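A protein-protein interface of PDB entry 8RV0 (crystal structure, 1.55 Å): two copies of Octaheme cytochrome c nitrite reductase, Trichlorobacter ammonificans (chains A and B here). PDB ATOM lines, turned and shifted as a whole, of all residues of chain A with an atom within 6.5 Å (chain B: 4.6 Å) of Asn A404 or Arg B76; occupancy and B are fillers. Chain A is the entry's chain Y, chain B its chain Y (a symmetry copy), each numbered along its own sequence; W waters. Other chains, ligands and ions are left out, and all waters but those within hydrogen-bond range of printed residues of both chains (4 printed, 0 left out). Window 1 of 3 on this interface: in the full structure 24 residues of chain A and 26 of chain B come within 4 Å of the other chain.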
ATOM      1  N   PHE A 397     -34.131  23.614 -22.764  1.00  0.00           N
ATOM      2  CA  PHE A 397     -33.404  22.720 -21.881  1.00  0.00           C
ATOM      3  C   PHE A 397     -31.974  23.207 -21.640  1.00  0.00           C
ATOM      4  O   PHE A 397     -31.531  23.188 -20.503  1.00  0.00           O
ATOM      5  CB  PHE A 397     -33.473  21.295 -22.462  1.00  0.00           C
ATOM      6  CG  PHE A 397     -32.612  20.333 -21.681  1.00  0.00           C
ATOM      7  CD1 PHE A 397     -33.166  19.548 -20.664  1.00  0.00           C
ATOM      8  CD2 PHE A 397     -31.268  20.195 -21.965  1.00  0.00           C
ATOM      9  CE1 PHE A 397     -32.336  18.606 -20.017  1.00  0.00           C
ATOM     10  CE2 PHE A 397     -30.479  19.239 -21.333  1.00  0.00           C
ATOM     11  CZ  PHE A 397     -30.993  18.442 -20.301  1.00  0.00           C
ATOM     12  N   ILE A 399     -30.641  26.259 -21.982  1.00  0.00           N
ATOM     13  CA  ILE A 399     -30.577  27.537 -21.268  1.00  0.00           C
ATOM     14  C   ILE A 399     -30.910  27.223 -19.813  1.00  0.00           C
ATOM     15  O   ILE A 399     -30.141  27.631 -18.916  1.00  0.00           O
ATOM     16  CB  ILE A 399     -31.586  28.545 -21.777  1.00  0.00           C
ATOM     17  CG1 ILE A 399     -31.278  28.878 -23.250  1.00  0.00           C
ATOM     18  CG2 ILE A 399     -31.599  29.749 -20.848  1.00  0.00           C
ATOM     19  CD1 ILE A 399     -32.432  29.654 -23.977  1.00  0.00           C
ATOM     20  N   GLU A 400     -31.996  26.451 -19.591  1.00  0.00           N
ATOM     21  CA  GLU A 400     -32.395  26.267 -18.200  1.00  0.00           C
ATOM     22  C   GLU A 400     -31.470  25.380 -17.395  1.00  0.00           C
ATOM     23  O   GLU A 400     -31.344  25.670 -16.196  1.00  0.00           O
ATOM     24  CB  GLU A 400     -33.828  25.747 -18.056  1.00  0.00           C
ATOM     25  CG  GLU A 400     -34.759  26.758 -18.607  1.00  0.00           C
ATOM     26  CD  GLU A 400     -35.008  28.037 -17.817  1.00  0.00           C
ATOM     27  OE1 GLU A 400     -34.178  28.433 -16.997  1.00  0.00           O
ATOM     28  OE2 GLU A 400     -35.984  28.626 -18.082  1.00  0.00           O
ATOM     29  N   THR A 401     -30.817  24.382 -18.025  1.00  0.00           N
ATOM     30  CA  THR A 401     -29.946  23.503 -17.224  1.00  0.00           C
ATOM     31  C   THR A 401     -28.785  24.305 -16.634  1.00  0.00           C
ATOM     32  O   THR A 401     -28.409  24.146 -15.445  1.00  0.00           O
ATOM     33  CB  THR A 401     -29.471  22.300 -18.074  1.00  0.00           C
ATOM     34  OG1 THR A 401     -30.661  21.560 -18.328  1.00  0.00           O
ATOM     35  CG2 THR A 401     -28.507  21.444 -17.296  1.00  0.00           C
ATOM     36  N   ILE A 402     -28.186  25.137 -17.491  1.00  0.00           N
ATOM     37  CA  ILE A 402     -27.054  25.959 -17.090  1.00  0.00           C
ATOM     38  C   ILE A 402     -27.474  26.933 -15.984  1.00  0.00           C
ATOM     39  O   ILE A 402     -26.760  27.107 -14.984  1.00  0.00           O
ATOM     40  CB  ILE A 402     -26.457  26.693 -18.302  1.00  0.00           C
ATOM     41  CG1 ILE A 402     -25.720  25.692 -19.213  1.00  0.00           C
ATOM     42  CG2 ILE A 402     -25.517  27.784 -17.729  1.00  0.00           C
ATOM     43  CD1 ILE A 402     -25.619  26.236 -20.606  1.00  0.00           C
ATOM     44  N   ARG A 403     -28.690  27.525 -16.145  1.00  0.00           N
ATOM     45  CA  ARG A 403     -29.119  28.479 -15.131  1.00  0.00           C
ATOM     46  C   ARG A 403     -29.434  27.715 -13.841  1.00  0.00           C
ATOM     47  O   ARG A 403     -29.170  28.192 -12.712  1.00  0.00           O
ATOM     48  CB  ARG A 403     -30.357  29.254 -15.586  1.00  0.00           C
ATOM     49  CG  ARG A 403     -30.005  30.283 -16.663  1.00  0.00           C
ATOM     50  CD  ARG A 403     -30.986  31.433 -16.940  1.00  0.00           C
ATOM     51  NE  ARG A 403     -32.350  30.967 -17.199  1.00  0.00           N
ATOM     52  CZ  ARG A 403     -33.366  31.794 -17.268  1.00  0.00           C
ATOM     53  NH1 ARG A 403     -34.579  31.291 -17.486  1.00  0.00           N
ATOM     54  NH2 ARG A 403     -33.149  33.102 -17.155  1.00  0.00           N
ATOM     55  N   ASN A 404     -29.952  26.476 -13.996  1.00  0.00           N
ATOM     56  CA  ASN A 404     -30.314  25.662 -12.863  1.00  0.00           C
ATOM     57  C   ASN A 404     -29.053  25.382 -12.020  1.00  0.00           C
ATOM     58  O   ASN A 404     -29.075  25.540 -10.788  1.00  0.00           O
ATOM     59  CB  ASN A 404     -30.962  24.315 -13.246  1.00  0.00           C
ATOM     60  CG  ASN A 404     -32.398  24.488 -13.765  1.00  0.00           C
ATOM     61  OD1 ASN A 404     -33.101  25.501 -13.471  1.00  0.00           O
ATOM     62  ND2 ASN A 404     -32.914  23.428 -14.430  1.00  0.00           N
ATOM     63  N   TYR A 405     -28.028  24.862 -12.692  1.00  0.00           N
ATOM     64  CA  TYR A 405     -26.801  24.525 -11.977  1.00  0.00           C
ATOM     65  C   TYR A 405     -26.152  25.802 -11.400  1.00  0.00           C
ATOM     66  O   TYR A 405     -25.757  25.821 -10.246  1.00  0.00           O
ATOM     67  CB  TYR A 405     -25.821  23.796 -12.923  1.00  0.00           C
ATOM     68  CG  TYR A 405     -24.517  23.451 -12.244  1.00  0.00           C
ATOM     69  CD1 TYR A 405     -24.426  22.315 -11.456  1.00  0.00           C
ATOM     70  CD2 TYR A 405     -23.434  24.313 -12.357  1.00  0.00           C
ATOM     71  CE1 TYR A 405     -23.235  21.989 -10.808  1.00  0.00           C
ATOM     72  CE2 TYR A 405     -22.218  23.986 -11.773  1.00  0.00           C
ATOM     73  CZ  TYR A 405     -22.143  22.835 -10.989  1.00  0.00           C
ATOM     74  OH  TYR A 405     -21.001  22.555 -10.292  1.00  0.00           O
ATOM     75  N   THR A 406     -26.146  26.882 -12.143  1.00  0.00           N
ATOM     76  CA  THR A 406     -25.558  28.162 -11.678  1.00  0.00           C
ATOM     77  C   THR A 406     -26.330  28.700 -10.460  1.00  0.00           C
ATOM     78  O   THR A 406     -25.784  29.065  -9.390  1.00  0.00           O
ATOM     79  CB  THR A 406     -25.473  29.219 -12.765  1.00  0.00           C
ATOM     80  OG1 THR A 406     -24.661  28.605 -13.770  1.00  0.00           O
ATOM     81  CG2 THR A 406     -24.678  30.408 -12.214  1.00  0.00           C
ATOM     82  N   LYS A 407     -27.623  28.746 -10.594  1.00  0.00           N
ATOM     83  CA  LYS A 407     -28.479  29.167  -9.475  1.00  0.00           C
ATOM     84  C   LYS A 407     -28.304  28.311  -8.209  1.00  0.00           C
ATOM     85  O   LYS A 407     -28.386  28.868  -7.108  1.00  0.00           O
ATOM     86  CB  LYS A 407     -29.942  29.329  -9.865  1.00  0.00           C
ATOM     87  CG  LYS A 407     -30.007  30.485 -10.866  1.00  0.00           C
ATOM     88  CD  LYS A 407     -31.463  30.865 -11.234  1.00  0.00           C
ATOM     89  CE  LYS A 407     -32.029  29.911 -12.198  1.00  0.00           C
ATOM     90  NZ  LYS A 407     -33.483  30.121 -12.364  1.00  0.00           N
ATOM     91  N   GLY A 408     -28.091  27.013  -8.328  1.00  0.00           N
ATOM     92  CA  GLY A 408     -27.870  26.216  -7.146  1.00  0.00           C
ATOM     93  C   GLY A 408     -26.642  26.741  -6.370  1.00  0.00           C
ATOM     94  O   GLY A 408     -26.677  26.812  -5.118  1.00  0.00           O
ATOM     95  N   LYS A 409     -25.589  27.146  -7.114  1.00  0.00           N
ATOM     96  CA  LYS A 409     -24.370  27.639  -6.454  1.00  0.00           C
ATOM     97  C   LYS A 409     -24.624  29.060  -5.964  1.00  0.00           C
ATOM     98  O   LYS A 409     -24.097  29.443  -4.923  1.00  0.00           O
ATOM     99  CB  LYS A 409     -23.209  27.603  -7.456  1.00  0.00           C
ATOM    100  CG  LYS A 409     -22.904  26.205  -7.937  1.00  0.00           C
ATOM    101  CD  LYS A 409     -22.795  25.166  -6.810  1.00  0.00           C
ATOM    102  CE  LYS A 409     -22.459  23.844  -7.456  1.00  0.00           C
ATOM    103  NZ  LYS A 409     -22.313  22.705  -6.524  1.00  0.00           N
ATOM    104  N   ASP A 460     -27.758  34.521 -15.191  1.00  0.00           N
ATOM    105  CA  ASP A 460     -27.678  33.361 -14.276  1.00  0.00           C
ATOM    106  C   ASP A 460     -26.728  32.275 -14.773  1.00  0.00           C
ATOM    107  O   ASP A 460     -27.002  31.078 -14.733  1.00  0.00           O
ATOM    108  CB  ASP A 460     -29.044  32.755 -13.955  1.00  0.00           C
ATOM    109  CG  ASP A 460     -29.859  33.650 -13.028  1.00  0.00           C
ATOM    110  OD1 ASP A 460     -29.340  34.005 -11.964  1.00  0.00           O
ATOM    111  OD2 ASP A 460     -30.958  34.059 -13.431  1.00  0.00           O
ATOM    112  N   THR B  73     -37.771  23.025 -18.694  1.00  0.00           N
ATOM    113  CA  THR B  73     -37.340  23.674 -17.440  1.00  0.00           C
ATOM    114  C   THR B  73     -35.913  23.211 -17.101  1.00  0.00           C
ATOM    115  O   THR B  73     -35.406  23.569 -16.083  1.00  0.00           O
ATOM    116  CB  THR B  73     -38.398  23.421 -16.350  1.00  0.00           C
ATOM    117  OG1 THR B  73     -38.374  22.033 -15.997  1.00  0.00           O
ATOM    118  CG2 THR B  73     -39.809  23.913 -16.707  1.00  0.00           C
ATOM    119  N   GLY B  74     -35.273  22.395 -17.938  1.00  0.00           N
ATOM    120  CA  GLY B  74     -33.918  21.917 -17.716  1.00  0.00           C
ATOM    121  C   GLY B  74     -33.826  20.752 -16.720  1.00  0.00           C
ATOM    122  O   GLY B  74     -34.789  20.260 -16.128  1.00  0.00           O
ATOM    123  N   ALA B  75     -32.584  20.348 -16.507  1.00  0.00           N
ATOM    124  CA  ALA B  75     -32.227  19.315 -15.521  1.00  0.00           C
ATOM    125  C   ALA B  75     -31.171  19.920 -14.587  1.00  0.00           C
ATOM    126  O   ALA B  75     -30.998  21.111 -14.593  1.00  0.00           O
ATOM    127  CB  ALA B  75     -31.783  18.042 -16.280  1.00  0.00           C
ATOM    128  N   ARG B  76     -30.405  19.080 -13.885  1.00  0.00           N
ATOM    129  CA  ARG B  76     -29.443  19.499 -12.891  1.00  0.00           C
ATOM    130  C   ARG B  76     -30.098  20.461 -11.886  1.00  0.00           C
ATOM    131  O   ARG B  76     -29.488  21.459 -11.479  1.00  0.00           O
ATOM    132  CB  ARG B  76     -28.117  19.843 -13.547  1.00  0.00           C
ATOM    133  CG  ARG B  76     -26.942  19.649 -12.615  1.00  0.00           C
ATOM    134  CD  ARG B  76     -25.737  18.978 -13.231  1.00  0.00           C
ATOM    135  NE  ARG B  76     -24.674  18.947 -12.225  1.00  0.00           N
ATOM    136  CZ  ARG B  76     -23.426  18.607 -12.561  1.00  0.00           C
ATOM    137  NH1 ARG B  76     -23.182  18.301 -13.833  1.00  0.00           N
ATOM    138  NH2 ARG B  76     -22.464  18.549 -11.624  1.00  0.00           N
ATOM    139  N   LYS B  77     -31.354  20.120 -11.487  1.00  0.00           N
ATOM    140  CA  LYS B  77     -32.119  21.006 -10.596  1.00  0.00           C
ATOM    141  C   LYS B  77     -31.669  20.755  -9.152  1.00  0.00           C
ATOM    142  O   LYS B  77     -32.116  19.812  -8.521  1.00  0.00           O
ATOM    143  CB  LYS B  77     -33.646  20.838 -10.640  1.00  0.00           C
ATOM    144  CG  LYS B  77     -34.187  20.997 -12.069  1.00  0.00           C
ATOM    145  CD  LYS B  77     -35.692  20.842 -12.133  1.00  0.00           C
ATOM    146  CE  LYS B  77     -36.130  21.291 -13.526  1.00  0.00           C
ATOM    147  NZ  LYS B  77     -37.526  20.871 -13.786  1.00  0.00           N
ATOM    148  N   GLU B  78     -30.844  21.653  -8.637  1.00  0.00           N
ATOM    149  CA  GLU B  78     -30.419  21.599  -7.235  1.00  0.00           C
ATOM    150  C   GLU B  78     -31.651  21.677  -6.313  1.00  0.00           C
ATOM    151  O   GLU B  78     -32.508  22.558  -6.463  1.00  0.00           O
ATOM    152  CB  GLU B  78     -29.322  22.653  -6.994  1.00  0.00           C
ATOM    153  CG  GLU B  78     -28.995  22.840  -5.537  1.00  0.00           C
ATOM    154  CD  GLU B  78     -28.362  21.672  -4.778  1.00  0.00           C
ATOM    155  OE1 GLU B  78     -27.386  21.020  -5.321  1.00  0.00           O
ATOM    156  OE2 GLU B  78     -28.870  21.424  -3.665  1.00  0.00           O
ATOM    157  N   GLU B 101     -23.696  19.155  -3.598  1.00  0.00           N
ATOM    158  CA  GLU B 101     -24.610  19.136  -4.757  1.00  0.00           C
ATOM    159  C   GLU B 101     -25.573  17.966  -4.613  1.00  0.00           C
ATOM    160  O   GLU B 101     -25.160  16.829  -4.388  1.00  0.00           O
ATOM    161  CB  GLU B 101     -23.934  18.959  -6.125  1.00  0.00           C
ATOM    162  CG  GLU B 101     -24.959  18.971  -7.237  1.00  0.00           C
ATOM    163  CD  GLU B 101     -24.419  19.079  -8.671  1.00  0.00           C
ATOM    164  OE1 GLU B 101     -23.185  18.778  -8.876  1.00  0.00           O
ATOM    165  OE2 GLU B 101     -25.210  19.438  -9.632  1.00  0.00           O
ATOM    166  N   ALA B 103     -29.237  17.093  -6.793  1.00  0.00           N
ATOM    167  CA  ALA B 103     -30.219  17.587  -7.749  1.00  0.00           C
ATOM    168  C   ALA B 103     -31.345  16.573  -7.828  1.00  0.00           C
ATOM    169  O   ALA B 103     -31.171  15.420  -7.413  1.00  0.00           O
ATOM    170  CB  ALA B 103     -29.642  17.767  -9.139  1.00  0.00           C
ATOM    171  N   ALA B 117     -20.511  12.437 -12.482  1.00  0.00           N
ATOM    172  CA  ALA B 117     -20.206  13.841 -12.761  1.00  0.00           C
ATOM    173  C   ALA B 117     -20.687  14.742 -11.609  1.00  0.00           C
ATOM    174  O   ALA B 117     -20.356  15.967 -11.552  1.00  0.00           O
ATOM    175  CB  ALA B 117     -20.909  14.233 -14.020  1.00  0.00           C
ATOM    176  N   VAL B 118     -21.531  14.228 -10.706  1.00  0.00           N
ATOM    177  CA  VAL B 118     -22.095  15.122  -9.691  1.00  0.00           C
ATOM    178  C   VAL B 118     -20.931  15.633  -8.817  1.00  0.00           C
ATOM    179  O   VAL B 118     -19.963  14.906  -8.588  1.00  0.00           O
ATOM    180  CB  VAL B 118     -23.208  14.418  -8.857  1.00  0.00           C
ATOM    181  CG1 VAL B 118     -22.556  13.361  -7.953  1.00  0.00           C
ATOM    182  CG2 VAL B 118     -24.001  15.394  -7.969  1.00  0.00           C
ATOM    183  N   ASP B 119     -21.098  16.852  -8.275  1.00  0.00           N
ATOM    184  CA  ASP B 119     -20.010  17.530  -7.528  1.00  0.00           C
ATOM    185  C   ASP B 119     -19.611  16.741  -6.285  1.00  0.00           C
ATOM    186  O   ASP B 119     -18.532  16.992  -5.798  1.00  0.00           O
ATOM    187  CB  ASP B 119     -20.266  18.988  -7.183  1.00  0.00           C
ATOM    188  CG  ASP B 119     -20.308  19.915  -8.397  1.00  0.00           C
ATOM    189  OD1 ASP B 119     -19.923  19.505  -9.455  1.00  0.00           O
ATOM    190  OD2 ASP B 119     -20.687  21.090  -8.202  1.00  0.00           O
ATOM    191  N   TRP B 132     -21.478  21.504 -21.429  1.00  0.00           N
ATOM    192  CA  TRP B 132     -22.926  21.568 -21.274  1.00  0.00           C
ATOM    193  C   TRP B 132     -23.653  21.184 -22.546  1.00  0.00           C
ATOM    194  O   TRP B 132     -24.754  20.671 -22.477  1.00  0.00           O
ATOM    195  CB  TRP B 132     -23.399  22.931 -20.803  1.00  0.00           C
ATOM    196  CG  TRP B 132     -23.069  23.186 -19.374  1.00  0.00           C
ATOM    197  CD1 TRP B 132     -22.186  24.102 -18.862  1.00  0.00           C
ATOM    198  CD2 TRP B 132     -23.670  22.482 -18.267  1.00  0.00           C
ATOM    199  NE1 TRP B 132     -22.311  24.054 -17.513  1.00  0.00           N
ATOM    200  CE2 TRP B 132     -23.119  23.031 -17.106  1.00  0.00           C
ATOM    201  CE3 TRP B 132     -24.669  21.505 -18.137  1.00  0.00           C
ATOM    202  CZ2 TRP B 132     -23.538  22.645 -15.820  1.00  0.00           C
ATOM    203  CZ3 TRP B 132     -25.049  21.086 -16.880  1.00  0.00           C
ATOM    204  CH2 TRP B 132     -24.478  21.644 -15.731  1.00  0.00           C
ATOM    205  N   TYR B 135     -24.721  17.624 -22.387  1.00  0.00           N
ATOM    206  CA  TYR B 135     -25.404  17.132 -21.204  1.00  0.00           C
ATOM    207  C   TYR B 135     -26.586  16.219 -21.479  1.00  0.00           C
ATOM    208  O   TYR B 135     -26.970  15.436 -20.597  1.00  0.00           O
ATOM    209  CB  TYR B 135     -25.898  18.354 -20.411  1.00  0.00           C
ATOM    210  CG  TYR B 135     -26.232  17.956 -18.994  1.00  0.00           C
ATOM    211  CD1 TYR B 135     -25.238  17.494 -18.140  1.00  0.00           C
ATOM    212  CD2 TYR B 135     -27.522  18.113 -18.494  1.00  0.00           C
ATOM    213  CE1 TYR B 135     -25.555  17.089 -16.821  1.00  0.00           C
ATOM    214  CE2 TYR B 135     -27.843  17.750 -17.166  1.00  0.00           C
ATOM    215  CZ  TYR B 135     -26.857  17.215 -16.363  1.00  0.00           C
ATOM    216  OH  TYR B 135     -27.151  16.874 -15.092  1.00  0.00           O
HETATM  217  O   HOH W   1     -25.235  22.615  -5.985  1.00  0.00           O
HETATM  218  O   HOH W   2     -35.838  25.561 -14.160  1.00  0.00           O
HETATM  219  O   HOH W   3     -31.471  24.931  -9.325  1.00  0.00           O
HETATM  220  O   HOH W   4     -19.509  20.415 -12.147  1.00  0.00           O
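OG1 of Thr A401 sits at hydrogen-bond distance from N of Ala B75 (2.9 Å). ND2 of Asn A404 is in hydrogen-bond range of O of Thr B73, 3.0 Å away. The side-chain amide nitrogen of Asn A404 lies within hydrogen-bond range of the backbone carbonyl oxygen of Ala B75 (3.0 Å). The side-chain carboxylate (OD2) of Asp B119 is in hydrogen-bond range of the side-chain hydroxyl (OH) of Tyr A405, 2.6 Å away. OD2 of Asp B119 lies within salt-bridge range of NZ of Lys A409.
Among the printed residues, pairs that only touch across the chains: Phe A397 with Gly B74 (3.9 Å), Phe A397 with Ala B75 (3.8 Å), Phe A397 with Tyr B135 (3.9 Å), Glu A400 with Thr B73 (3.3 Å), Glu A400 with Gly B74 (3.7 Å), Thr A401 with Gly B74 (3.3 Å), Thr A401 with Trp B132 (3.5 Å), Thr A401 with Tyr B135 (3.7 Å), Ile A402 with Trp B132 (3.7 Å), Asn A404 with Gly B74 (3.6 Å), Asn A404 with Arg B76 (3.7 Å), Asn A404 with Lys B77 (3.6 Å), Tyr A405 with Arg B76 (3.5 Å), Tyr A405 with Glu B101 (3.4 Å), Tyr A405 with Trp B132 (3.8 Å) and Gly A408 with Glu B78 (3.9 Å).
Water W1 bridges the side-chain carboxylate of Glu B78 (2.8 Å) and the side-chain amino group of Lys A409 (3.0 Å). Water W2 bridges O of Thr B73 (2.8 Å) and OD1 of Asn A404 (2.8 Å). Water W4 lies within hydrogen-bond range of the side-chain carboxylate of Asp B119 and the side-chain hydroxyl of Tyr A405. Water W3 lies within hydrogen-bond range of O of Asn A404 (2.9 Å) and N of Glu B78 (3.4 Å).
O of Phe A397 lies within hydrogen-bond range of OG1 of Thr A401 (2.9 Å). O of Ile A402 is in hydrogen-bond range of OG1 of Thr A406 (2.9 Å). OG1 of Thr B73 lies within hydrogen-bond range of NZ of Lys B77 (2.6 Å). The guanidinium group of Arg B76 is in hydrogen-bond range of the backbone carbonyl oxygen of Ala B117 (3.3 Å). The guanidinium group (NH2) of Arg B76 is in salt-bridge range of the side-chain carboxylate (OD1) of Asp B119 (3.5 Å). N of Asp B119 lies within hydrogen-bond range of OE1 of Glu B101.
Printed residues of chain B within 4 Å of Asn A404: Thr B73 (3.0 Å), Gly B74 (3.6 Å), Ala B75 (3.0 Å), Arg B76 (3.7 Å) and Lys B77 (3.6 Å). Arg B76 touches just these residues of chain A: Asn A404 and Tyr A405. Of the printed residues of chain B, Glu A400 touches Thr B73 (3.3 Å) and Gly B74 (3.7 Å). Printed residues of chain A within 4 Å of Glu B78: Gly A408. Printed residues of chain A within 4 Å of Gly B74: Phe A397, Glu A400, Thr A401 and Asn A404. Of the printed residues of chain A, Glu B101 touches Tyr A405. Of the printed residues of chain B, Gly A408 touches Glu B78. Asp A460 touches none of the printed residues of chain B. Ala B103 touches none of the printed residues of chain A. The nearest printed residue of chain B that does not touch Asn A404 is Glu B78 (4.8 Å). The nearest residue of chain A that does not touch Arg B76 is Thr A401 (4.1 Å).
Printed residues of chain A that touch a printed residue of chain B: Phe A397, Glu A400, Thr A401, Ile A402, Asn A404, Tyr A405, Gly A408 and Lys A409. Hydrophobic or aromatic side chains of chain A within 4 Å of the printed part of chain B: Phe A397, Ile A402 and Tyr A405. Hydrophobic or aromatic side chains of chain B within 4 Å of the printed part of chain A: Ala B75, Trp B132 and Tyr B135. Among the printed residues, 21 pairs touch across the chains.
No position is printed for both chains. Of the 21 pairs that touch across the chains among the printed residues, none has its exchanged pair printed and touching as well.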
